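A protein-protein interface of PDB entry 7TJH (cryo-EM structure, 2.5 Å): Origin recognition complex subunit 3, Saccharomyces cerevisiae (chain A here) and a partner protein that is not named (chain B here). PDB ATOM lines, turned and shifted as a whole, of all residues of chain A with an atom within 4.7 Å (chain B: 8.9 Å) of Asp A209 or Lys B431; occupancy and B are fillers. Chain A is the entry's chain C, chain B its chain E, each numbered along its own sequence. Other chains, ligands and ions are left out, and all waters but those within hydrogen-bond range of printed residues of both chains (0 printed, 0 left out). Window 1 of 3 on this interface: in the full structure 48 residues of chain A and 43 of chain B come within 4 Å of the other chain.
The backbone carbonyl oxygen of Ile A211 lies within hydrogen-bond range of the side-chain amino group of Lys B431.
The backbone carbonyl oxygen (O) of Leu B430 lies close to the backbone carbonyl oxygen (O) of Asp A209, at 3.3 Å.
The side-chain carboxylate (OD1) of Asp A209 lies within hydrogen-bond range of the backbone NH (N) of Asn A241, at 2.9 Å.
The side-chain carboxylate (OD2) of Asp A209 is in hydrogen-bond range of the side-chain hydroxyl (OG1) of Thr A242 (2.6 Å).
OG1 of Thr B429 lies within hydrogen-bond range of O of Ser B425, at 2.9 Å.
O of Leu B427 sits at hydrogen-bond distance from N of Leu B432.
The backbone carbonyl oxygen (O) of Lys B431 sits at hydrogen-bond distance from the side-chain amide nitrogen (ND2) of Asn B453 (3.2 Å).
The backbone carbonyl oxygen (O) of Leu B432 is in hydrogen-bond range of the backbone NH (N) of Asn B453 (2.9 Å).
Asp A209 touches Lys B431 (O to CE, 3.3 Å).
Thr B429 touches Ser A210.
CE of Lys B431 touches C of Ser A210, at 3.5 Å.
CD2 of Phe A213 touches NZ of Lys B431, at 3.9 Å.
CB of Asn A241 touches CD2 of Leu B430 (3.8 Å).
CD1 of Leu B430 touches CG2 of Thr A242, at 3.8 Å.
CG2 of Thr A242 touches CD2 of Leu B432, 3.9 Å away.
Asp A209 touches two residues of chain B.
Of chain A, only Asp A209 (3.3 Å), Ser A210 (3.5 Å), Ile A211 (2.8 Å) and Phe A213 (3.9 Å) come within 4 Å of Lys B431.
Printed residues of chain A within 4 Å of Thr B429: Ser A210 (3.5 Å).
Printed residues of chain B within 4 Å of Thr A242: Leu B430 and Leu B432.
Printed residues of chain A within 4 Å of Leu B432: Thr A242 (3.9 Å).
Of the printed residues of chain B, Phe A213 touches Lys B431 (3.9 Å).
Of the printed residues of chain A, Leu B430 touches Asp A209 (3.3 Å), Asn A241 (3.8 Å) and Thr A242 (3.8 Å).
Val B452 touches none of the printed residues of chain A.
Of the 11 printed residues of chain A, 6 touch a printed residue of chain B.
Printed residues of chain A that touch a printed residue of chain B: Asp A209, Ser A210, Ile A211, Phe A213, Asn A241 and Thr A242.
Of the 21 printed residues of chain B, 4 touch a printed residue of chain A.
Hydrophobic or aromatic side chains of chain B that line the printed part of chain A: Leu B430 and Leu B432.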
ATOM      1  N   ASP A 207      16.633  -7.682  -7.161  1.00  0.00           N
ATOM      2  CA  ASP A 207      15.173  -7.589  -6.997  1.00  0.00           C
ATOM      3  C   ASP A 207      14.595  -8.826  -6.302  1.00  0.00           C
ATOM      4  O   ASP A 207      13.849  -9.610  -6.891  1.00  0.00           O
ATOM      5  CB  ASP A 207      14.481  -7.346  -8.344  1.00  0.00           C
ATOM      6  CG  ASP A 207      14.879  -6.028  -8.979  1.00  0.00           C
ATOM      7  OD1 ASP A 207      15.873  -6.006  -9.734  1.00  0.00           O
ATOM      8  OD2 ASP A 207      14.194  -5.013  -8.733  1.00  0.00           O
ATOM      9  N   VAL A 208      14.979  -8.995  -5.033  1.00  0.00           N
ATOM     10  CA  VAL A 208      14.624 -10.185  -4.257  1.00  0.00           C
ATOM     11  C   VAL A 208      13.119 -10.256  -4.021  1.00  0.00           C
ATOM     12  O   VAL A 208      12.529 -11.344  -4.020  1.00  0.00           O
ATOM     13  CB  VAL A 208      15.425 -10.192  -2.939  1.00  0.00           C
ATOM     14  CG1 VAL A 208      15.042 -11.364  -2.035  1.00  0.00           C
ATOM     15  CG2 VAL A 208      16.900 -10.227  -3.235  1.00  0.00           C
ATOM     16  N   ASP A 209      12.456  -9.107  -3.912  1.00  0.00           N
ATOM     17  CA  ASP A 209      11.016  -9.055  -3.692  1.00  0.00           C
ATOM     18  C   ASP A 209      10.195  -9.477  -4.912  1.00  0.00           C
ATOM     19  O   ASP A 209       8.965  -9.458  -4.828  1.00  0.00           O
ATOM     20  CB  ASP A 209      10.623  -7.643  -3.257  1.00  0.00           C
ATOM     21  CG  ASP A 209      11.474  -7.137  -2.109  1.00  0.00           C
ATOM     22  OD1 ASP A 209      12.713  -7.097  -2.265  1.00  0.00           O
ATOM     23  OD2 ASP A 209      10.913  -6.786  -1.052  1.00  0.00           O
ATOM     24  N   SER A 210      10.832  -9.832  -6.033  1.00  0.00           N
ATOM     25  CA  SER A 210      10.160 -10.398  -7.192  1.00  0.00           C
ATOM     26  C   SER A 210      10.454 -11.879  -7.408  1.00  0.00           C
ATOM     27  O   SER A 210       9.827 -12.491  -8.278  1.00  0.00           O
ATOM     28  CB  SER A 210      10.544  -9.622  -8.460  1.00  0.00           C
ATOM     29  OG  SER A 210      10.319  -8.232  -8.296  1.00  0.00           O
ATOM     30  N   ILE A 211      11.380 -12.469  -6.652  1.00  0.00           N
ATOM     31  CA  ILE A 211      11.793 -13.849  -6.890  1.00  0.00           C
ATOM     32  C   ILE A 211      10.841 -14.806  -6.181  1.00  0.00           C
ATOM     33  O   ILE A 211      10.148 -14.443  -5.222  1.00  0.00           O
ATOM     34  CB  ILE A 211      13.261 -14.062  -6.453  1.00  0.00           C
ATOM     35  CG1 ILE A 211      13.920 -15.181  -7.264  1.00  0.00           C
ATOM     36  CG2 ILE A 211      13.379 -14.374  -4.961  1.00  0.00           C
ATOM     37  CD1 ILE A 211      15.395 -15.333  -7.006  1.00  0.00           C
ATOM     38  N   ASN A 212      10.767 -16.031  -6.694  1.00  0.00           N
ATOM     39  CA  ASN A 212      10.075 -17.107  -6.000  1.00  0.00           C
ATOM     40  C   ASN A 212      10.904 -17.541  -4.800  1.00  0.00           C
ATOM     41  O   ASN A 212      12.038 -18.007  -4.958  1.00  0.00           O
ATOM     42  CB  ASN A 212       9.843 -18.281  -6.945  1.00  0.00           C
ATOM     43  CG  ASN A 212       8.636 -19.104  -6.562  1.00  0.00           C
ATOM     44  OD1 ASN A 212       8.715 -19.974  -5.698  1.00  0.00           O
ATOM     45  ND2 ASN A 212       7.513 -18.842  -7.212  1.00  0.00           N
ATOM     46  N   PHE A 213      10.342 -17.387  -3.600  1.00  0.00           N
ATOM     47  CA  PHE A 213      11.115 -17.620  -2.387  1.00  0.00           C
ATOM     48  C   PHE A 213      11.370 -19.096  -2.120  1.00  0.00           C
ATOM     49  O   PHE A 213      12.339 -19.422  -1.431  1.00  0.00           O
ATOM     50  CB  PHE A 213      10.419 -16.971  -1.193  1.00  0.00           C
ATOM     51  CG  PHE A 213      10.687 -15.502  -1.075  1.00  0.00           C
ATOM     52  CD1 PHE A 213      11.875 -15.048  -0.528  1.00  0.00           C
ATOM     53  CD2 PHE A 213       9.759 -14.576  -1.522  1.00  0.00           C
ATOM     54  CE1 PHE A 213      12.133 -13.692  -0.420  1.00  0.00           C
ATOM     55  CE2 PHE A 213      10.007 -13.221  -1.418  1.00  0.00           C
ATOM     56  CZ  PHE A 213      11.198 -12.778  -0.866  1.00  0.00           C
ATOM     57  N   ASN A 239      18.961  -7.673  -2.338  1.00  0.00           N
ATOM     58  CA  ASN A 239      18.445  -6.325  -2.573  1.00  0.00           C
ATOM     59  C   ASN A 239      16.959  -6.320  -2.231  1.00  0.00           C
ATOM     60  O   ASN A 239      16.119  -6.718  -3.039  1.00  0.00           O
ATOM     61  CB  ASN A 239      18.696  -5.899  -4.016  1.00  0.00           C
ATOM     62  CG  ASN A 239      20.172  -5.809  -4.349  1.00  0.00           C
ATOM     63  OD1 ASN A 239      20.786  -4.756  -4.207  1.00  0.00           O
ATOM     64  ND2 ASN A 239      20.749  -6.917  -4.787  1.00  0.00           N
ATOM     65  N   ILE A 240      16.636  -5.859  -1.024  1.00  0.00           N
ATOM     66  CA  ILE A 240      15.283  -5.898  -0.484  1.00  0.00           C
ATOM     67  C   ILE A 240      14.639  -4.535  -0.683  1.00  0.00           C
ATOM     68  O   ILE A 240      15.255  -3.502  -0.395  1.00  0.00           O
ATOM     69  CB  ILE A 240      15.296  -6.280   1.006  1.00  0.00           C
ATOM     70  CG1 ILE A 240      16.185  -7.504   1.235  1.00  0.00           C
ATOM     71  CG2 ILE A 240      13.882  -6.521   1.518  1.00  0.00           C
ATOM     72  CD1 ILE A 240      15.670  -8.756   0.588  1.00  0.00           C
ATOM     73  N   ASN A 241      13.400  -4.525  -1.168  1.00  0.00           N
ATOM     74  CA  ASN A 241      12.674  -3.280  -1.352  1.00  0.00           C
ATOM     75  C   ASN A 241      11.492  -3.098  -0.412  1.00  0.00           C
ATOM     76  O   ASN A 241      10.941  -1.994  -0.362  1.00  0.00           O
ATOM     77  CB  ASN A 241      12.176  -3.154  -2.798  1.00  0.00           C
ATOM     78  CG  ASN A 241      13.192  -2.503  -3.708  1.00  0.00           C
ATOM     79  OD1 ASN A 241      13.995  -1.678  -3.273  1.00  0.00           O
ATOM     80  ND2 ASN A 241      13.155  -2.860  -4.984  1.00  0.00           N
ATOM     81  N   THR A 242      11.065  -4.131   0.318  1.00  0.00           N
ATOM     82  CA  THR A 242       9.918  -3.923   1.195  1.00  0.00           C
ATOM     83  C   THR A 242      10.304  -3.748   2.661  1.00  0.00           C
ATOM     84  O   THR A 242      10.183  -2.639   3.195  1.00  0.00           O
ATOM     85  CB  THR A 242       8.931  -5.086   1.061  1.00  0.00           C
ATOM     86  OG1 THR A 242       9.638  -6.330   1.132  1.00  0.00           O
ATOM     87  CG2 THR A 242       8.186  -5.004  -0.263  1.00  0.00           C
ATOM     88  N   LEU B 324       7.805   2.156   3.041  1.00  0.00           N
ATOM     89  CA  LEU B 324       6.782   2.304   2.013  1.00  0.00           C
ATOM     90  C   LEU B 324       6.114   3.673   2.087  1.00  0.00           C
ATOM     91  O   LEU B 324       6.068   4.313   3.141  1.00  0.00           O
ATOM     92  CB  LEU B 324       5.726   1.207   2.146  1.00  0.00           C
ATOM     93  CG  LEU B 324       5.401   0.410   0.882  1.00  0.00           C
ATOM     94  CD1 LEU B 324       6.672  -0.079   0.206  1.00  0.00           C
ATOM     95  CD2 LEU B 324       4.478  -0.755   1.209  1.00  0.00           C
ATOM     96  N   LEU B 332      -2.441  -0.594   0.312  1.00  0.00           N
ATOM     97  CA  LEU B 332      -2.362  -1.935   0.888  1.00  0.00           C
ATOM     98  C   LEU B 332      -3.460  -2.171   1.917  1.00  0.00           C
ATOM     99  O   LEU B 332      -4.030  -3.267   1.976  1.00  0.00           O
ATOM    100  CB  LEU B 332      -0.991  -2.166   1.520  1.00  0.00           C
ATOM    101  CG  LEU B 332       0.032  -2.936   0.688  1.00  0.00           C
ATOM    102  CD1 LEU B 332       1.246  -3.281   1.529  1.00  0.00           C
ATOM    103  CD2 LEU B 332      -0.582  -4.193   0.082  1.00  0.00           C
ATOM    104  N   LEU B 424       0.188   1.743  -7.109  1.00  0.00           N
ATOM    105  CA  LEU B 424      -0.471   0.450  -7.262  1.00  0.00           C
ATOM    106  C   LEU B 424       0.347  -0.494  -8.140  1.00  0.00           C
ATOM    107  O   LEU B 424       0.456  -1.695  -7.847  1.00  0.00           O
ATOM    108  CB  LEU B 424      -1.870   0.659  -7.837  1.00  0.00           C
ATOM    109  CG  LEU B 424      -2.811  -0.540  -7.920  1.00  0.00           C
ATOM    110  CD1 LEU B 424      -2.865  -1.281  -6.597  1.00  0.00           C
ATOM    111  CD2 LEU B 424      -4.196  -0.087  -8.353  1.00  0.00           C
ATOM    112  N   SER B 425       0.940   0.037  -9.214  1.00  0.00           N
ATOM    113  CA  SER B 425       1.789  -0.771 -10.085  1.00  0.00           C
ATOM    114  C   SER B 425       3.047  -1.244  -9.360  1.00  0.00           C
ATOM    115  O   SER B 425       3.467  -2.397  -9.526  1.00  0.00           O
ATOM    116  CB  SER B 425       2.148   0.026 -11.341  1.00  0.00           C
ATOM    117  OG  SER B 425       3.006  -0.714 -12.190  1.00  0.00           O
ATOM    118  N   GLU B 426       3.653  -0.372  -8.543  1.00  0.00           N
ATOM    119  CA  GLU B 426       4.793  -0.788  -7.726  1.00  0.00           C
ATOM    120  C   GLU B 426       4.394  -1.818  -6.681  1.00  0.00           C
ATOM    121  O   GLU B 426       5.177  -2.720  -6.364  1.00  0.00           O
ATOM    122  CB  GLU B 426       5.439   0.415  -7.046  1.00  0.00           C
ATOM    123  CG  GLU B 426       6.560   0.999  -7.846  1.00  0.00           C
ATOM    124  CD  GLU B 426       7.858   0.243  -7.645  1.00  0.00           C
ATOM    125  OE1 GLU B 426       7.993  -0.432  -6.603  1.00  0.00           O
ATOM    126  OE2 GLU B 426       8.729   0.301  -8.537  1.00  0.00           O
ATOM    127  N   LEU B 427       3.190  -1.683  -6.125  1.00  0.00           N
ATOM    128  CA  LEU B 427       2.698  -2.635  -5.139  1.00  0.00           C
ATOM    129  C   LEU B 427       2.491  -4.009  -5.762  1.00  0.00           C
ATOM    130  O   LEU B 427       2.719  -5.036  -5.112  1.00  0.00           O
ATOM    131  CB  LEU B 427       1.404  -2.099  -4.533  1.00  0.00           C
ATOM    132  CG  LEU B 427       1.263  -2.044  -3.016  1.00  0.00           C
ATOM    133  CD1 LEU B 427       2.515  -1.477  -2.371  1.00  0.00           C
ATOM    134  CD2 LEU B 427       0.068  -1.181  -2.676  1.00  0.00           C
ATOM    135  N   HIS B 428       2.066  -4.045  -7.028  1.00  0.00           N
ATOM    136  CA  HIS B 428       2.014  -5.321  -7.734  1.00  0.00           C
ATOM    137  C   HIS B 428       3.413  -5.834  -8.065  1.00  0.00           C
ATOM    138  O   HIS B 428       3.624  -7.052  -8.112  1.00  0.00           O
ATOM    139  CB  HIS B 428       1.169  -5.201  -9.003  1.00  0.00           C
ATOM    140  CG  HIS B 428       1.032  -6.485  -9.763  1.00  0.00           C
ATOM    141  ND1 HIS B 428       2.004  -6.962 -10.616  1.00  0.00           N
ATOM    142  CD2 HIS B 428       0.039  -7.405  -9.778  1.00  0.00           C
ATOM    143  CE1 HIS B 428       1.616  -8.117 -11.124  1.00  0.00           C
ATOM    144  NE2 HIS B 428       0.424  -8.405 -10.636  1.00  0.00           N
ATOM    145  N   THR B 429       4.367  -4.931  -8.319  1.00  0.00           N
ATOM    146  CA  THR B 429       5.738  -5.341  -8.630  1.00  0.00           C
ATOM    147  C   THR B 429       6.404  -6.028  -7.437  1.00  0.00           C
ATOM    148  O   THR B 429       7.104  -7.035  -7.599  1.00  0.00           O
ATOM    149  CB  THR B 429       6.547  -4.122  -9.088  1.00  0.00           C
ATOM    150  OG1 THR B 429       5.972  -3.594 -10.289  1.00  0.00           O
ATOM    151  CG2 THR B 429       8.002  -4.476  -9.358  1.00  0.00           C
ATOM    152  N   LEU B 430       6.152  -5.531  -6.227  1.00  0.00           N
ATOM    153  CA  LEU B 430       6.728  -6.079  -5.003  1.00  0.00           C
ATOM    154  C   LEU B 430       6.007  -7.327  -4.498  1.00  0.00           C
ATOM    155  O   LEU B 430       6.427  -7.886  -3.480  1.00  0.00           O
ATOM    156  CB  LEU B 430       6.724  -5.003  -3.913  1.00  0.00           C
ATOM    157  CG  LEU B 430       7.506  -3.729  -4.240  1.00  0.00           C
ATOM    158  CD1 LEU B 430       7.382  -2.699  -3.128  1.00  0.00           C
ATOM    159  CD2 LEU B 430       8.965  -4.041  -4.527  1.00  0.00           C
ATOM    160  N   LYS B 431       4.952  -7.763  -5.196  1.00  0.00           N
ATOM    161  CA  LYS B 431       4.028  -8.836  -4.787  1.00  0.00           C
ATOM    162  C   LYS B 431       3.430  -8.609  -3.400  1.00  0.00           C
ATOM    163  O   LYS B 431       3.245  -9.545  -2.623  1.00  0.00           O
ATOM    164  CB  LYS B 431       4.648 -10.237  -4.859  1.00  0.00           C
ATOM    165  CG  LYS B 431       5.605 -10.547  -5.985  1.00  0.00           C
ATOM    166  CD  LYS B 431       5.995 -12.018  -5.856  1.00  0.00           C
ATOM    167  CE  LYS B 431       7.454 -12.244  -5.563  1.00  0.00           C
ATOM    168  NZ  LYS B 431       7.662 -13.385  -4.630  1.00  0.00           N
ATOM    169  N   LEU B 432       2.976  -7.405  -3.108  1.00  0.00           N
ATOM    170  CA  LEU B 432       2.227  -7.124  -1.861  1.00  0.00           C
ATOM    171  C   LEU B 432       0.768  -7.244  -2.259  1.00  0.00           C
ATOM    172  O   LEU B 432      -0.068  -7.499  -1.437  1.00  0.00           O
ATOM    173  CB  LEU B 432       2.611  -5.731  -1.377  1.00  0.00           C
ATOM    174  CG  LEU B 432       4.105  -5.530  -1.135  1.00  0.00           C
ATOM    175  CD1 LEU B 432       4.382  -4.166  -0.530  1.00  0.00           C
ATOM    176  CD2 LEU B 432       4.669  -6.626  -0.248  1.00  0.00           C
ATOM    177  N   ILE B 433       0.496  -7.044  -3.527  1.00  0.00           N
ATOM    178  CA  ILE B 433      -0.855  -7.291  -4.072  1.00  0.00           C
ATOM    179  C   ILE B 433      -0.585  -8.307  -5.169  1.00  0.00           C
ATOM    180  O   ILE B 433       0.538  -8.342  -5.673  1.00  0.00           O
ATOM    181  CB  ILE B 433      -1.545  -6.010  -4.575  1.00  0.00           C
ATOM    182  CG1 ILE B 433      -0.740  -5.366  -5.702  1.00  0.00           C
ATOM    183  CG2 ILE B 433      -1.836  -5.049  -3.439  1.00  0.00           C
ATOM    184  CD1 ILE B 433      -1.448  -4.252  -6.402  1.00  0.00           C
ATOM    185  N   ALA B 434      -1.569  -9.101  -5.537  1.00  0.00           N
ATOM    186  CA  ALA B 434      -1.340 -10.041  -6.659  1.00  0.00           C
ATOM    187  C   ALA B 434      -2.557 -10.179  -7.557  1.00  0.00           C
ATOM    188  O   ALA B 434      -3.603  -9.678  -7.238  1.00  0.00           O
ATOM    189  CB  ALA B 434      -0.928 -11.379  -6.126  1.00  0.00           C
ATOM    190  N   THR B 435      -2.372 -10.847  -8.678  1.00  0.00           N
ATOM    191  CA  THR B 435      -3.461 -11.022  -9.624  1.00  0.00           C
ATOM    192  C   THR B 435      -3.705 -12.507  -9.856  1.00  0.00           C
ATOM    193  O   THR B 435      -2.983 -13.368  -9.349  1.00  0.00           O
ATOM    194  CB  THR B 435      -3.163 -10.323 -10.957  1.00  0.00           C
ATOM    195  OG1 THR B 435      -1.809 -10.584 -11.347  1.00  0.00           O
ATOM    196  CG2 THR B 435      -3.363  -8.826 -10.829  1.00  0.00           C
ATOM    197  N   ASN B 438      -0.036 -14.747 -13.331  1.00  0.00           N
ATOM    198  CA  ASN B 438       1.302 -14.450 -12.832  1.00  0.00           C
ATOM    199  C   ASN B 438       2.286 -14.034 -13.917  1.00  0.00           C
ATOM    200  O   ASN B 438       3.183 -13.230 -13.642  1.00  0.00           O
ATOM    201  CB  ASN B 438       1.867 -15.662 -12.082  1.00  0.00           C
ATOM    202  CG  ASN B 438       0.999 -16.077 -10.914  1.00  0.00           C
ATOM    203  OD1 ASN B 438       0.627 -15.253 -10.081  1.00  0.00           O
ATOM    204  ND2 ASN B 438       0.665 -17.359 -10.849  1.00  0.00           N
ATOM    205  N   TYR B 443      -2.719  -6.060 -17.672  1.00  0.00           N
ATOM    206  CA  TYR B 443      -3.123  -5.186 -16.572  1.00  0.00           C
ATOM    207  C   TYR B 443      -4.463  -4.514 -16.848  1.00  0.00           C
ATOM    208  O   TYR B 443      -5.268  -4.317 -15.932  1.00  0.00           O
ATOM    209  CB  TYR B 443      -2.054  -4.121 -16.333  1.00  0.00           C
ATOM    210  CG  TYR B 443      -0.976  -4.483 -15.339  1.00  0.00           C
ATOM    211  CD1 TYR B 443      -1.218  -5.378 -14.302  1.00  0.00           C
ATOM    212  CD2 TYR B 443       0.287  -3.910 -15.430  1.00  0.00           C
ATOM    213  CE1 TYR B 443      -0.226  -5.699 -13.392  1.00  0.00           C
ATOM    214  CE2 TYR B 443       1.282  -4.219 -14.527  1.00  0.00           C
ATOM    215  CZ  TYR B 443       1.023  -5.113 -13.510  1.00  0.00           C
ATOM    216  OH  TYR B 443       2.022  -5.418 -12.616  1.00  0.00           O
ATOM    217  N   LYS B 451      -5.966  -9.262  -5.705  1.00  0.00           N
ATOM    218  CA  LYS B 451      -6.100  -9.674  -4.314  1.00  0.00           C
ATOM    219  C   LYS B 451      -4.901  -9.169  -3.527  1.00  0.00           C
ATOM    220  O   LYS B 451      -3.840  -8.893  -4.086  1.00  0.00           O
ATOM    221  CB  LYS B 451      -6.217 -11.197  -4.173  1.00  0.00           C
ATOM    222  CG  LYS B 451      -5.094 -11.967  -4.837  1.00  0.00           C
ATOM    223  CD  LYS B 451      -5.296 -13.461  -4.697  1.00  0.00           C
ATOM    224  CE  LYS B 451      -4.357 -14.228  -5.607  1.00  0.00           C
ATOM    225  NZ  LYS B 451      -4.155 -15.621  -5.135  1.00  0.00           N
ATOM    226  N   VAL B 452      -5.084  -9.039  -2.211  1.00  0.00           N
ATOM    227  CA  VAL B 452      -3.962  -8.715  -1.341  1.00  0.00           C
ATOM    228  C   VAL B 452      -3.070  -9.947  -1.208  1.00  0.00           C
ATOM    229  O   VAL B 452      -3.509 -11.089  -1.405  1.00  0.00           O
ATOM    230  CB  VAL B 452      -4.458  -8.199   0.028  1.00  0.00           C
ATOM    231  CG1 VAL B 452      -4.875  -9.340   0.961  1.00  0.00           C
ATOM    232  CG2 VAL B 452      -3.416  -7.306   0.698  1.00  0.00           C
ATOM    233  N   ASN B 453      -1.786  -9.718  -0.931  1.00  0.00           N
ATOM    234  CA  ASN B 453      -0.814 -10.799  -0.827  1.00  0.00           C
ATOM    235  C   ASN B 453       0.059 -10.637   0.411  1.00  0.00           C
ATOM    236  O   ASN B 453       1.188 -11.133   0.452  1.00  0.00           O
ATOM    237  CB  ASN B 453       0.042 -10.883  -2.091  1.00  0.00           C
ATOM    238  CG  ASN B 453       0.582 -12.286  -2.348  1.00  0.00           C
ATOM    239  OD1 ASN B 453      -0.073 -13.284  -2.045  1.00  0.00           O
ATOM    240  ND2 ASN B 453       1.781 -12.360  -2.904  1.00  0.00           N
ATOM    241  N   VAL B 454      -0.443  -9.943   1.429  1.00  0.00           N
ATOM    242  CA  VAL B 454       0.280  -9.799   2.692  1.00  0.00           C
ATOM    243  C   VAL B 454      -0.504 -10.502   3.799  1.00  0.00           C
ATOM    244  O   VAL B 454      -1.731 -10.656   3.691  1.00  0.00           O
ATOM    245  CB  VAL B 454       0.558  -8.317   3.022  1.00  0.00           C
ATOM    246  CG1 VAL B 454       1.076  -7.576   1.798  1.00  0.00           C
ATOM    247  CG2 VAL B 454      -0.677  -7.607   3.570  1.00  0.00           C
ATOM    248  N   PRO B 455       0.157 -11.003   4.838  1.00  0.00           N
ATOM    249  CA  PRO B 455      -0.565 -11.544   5.995  1.00  0.00           C
ATOM    250  C   PRO B 455      -1.075 -10.430   6.905  1.00  0.00           C
ATOM    251  O   PRO B 455      -0.802  -9.246   6.701  1.00  0.00           O
ATOM    252  CB  PRO B 455       0.488 -12.403   6.709  1.00  0.00           C
ATOM    253  CG  PRO B 455       1.596 -12.574   5.725  1.00  0.00           C
ATOM    254  CD  PRO B 455       1.587 -11.351   4.879  1.00  0.00           C
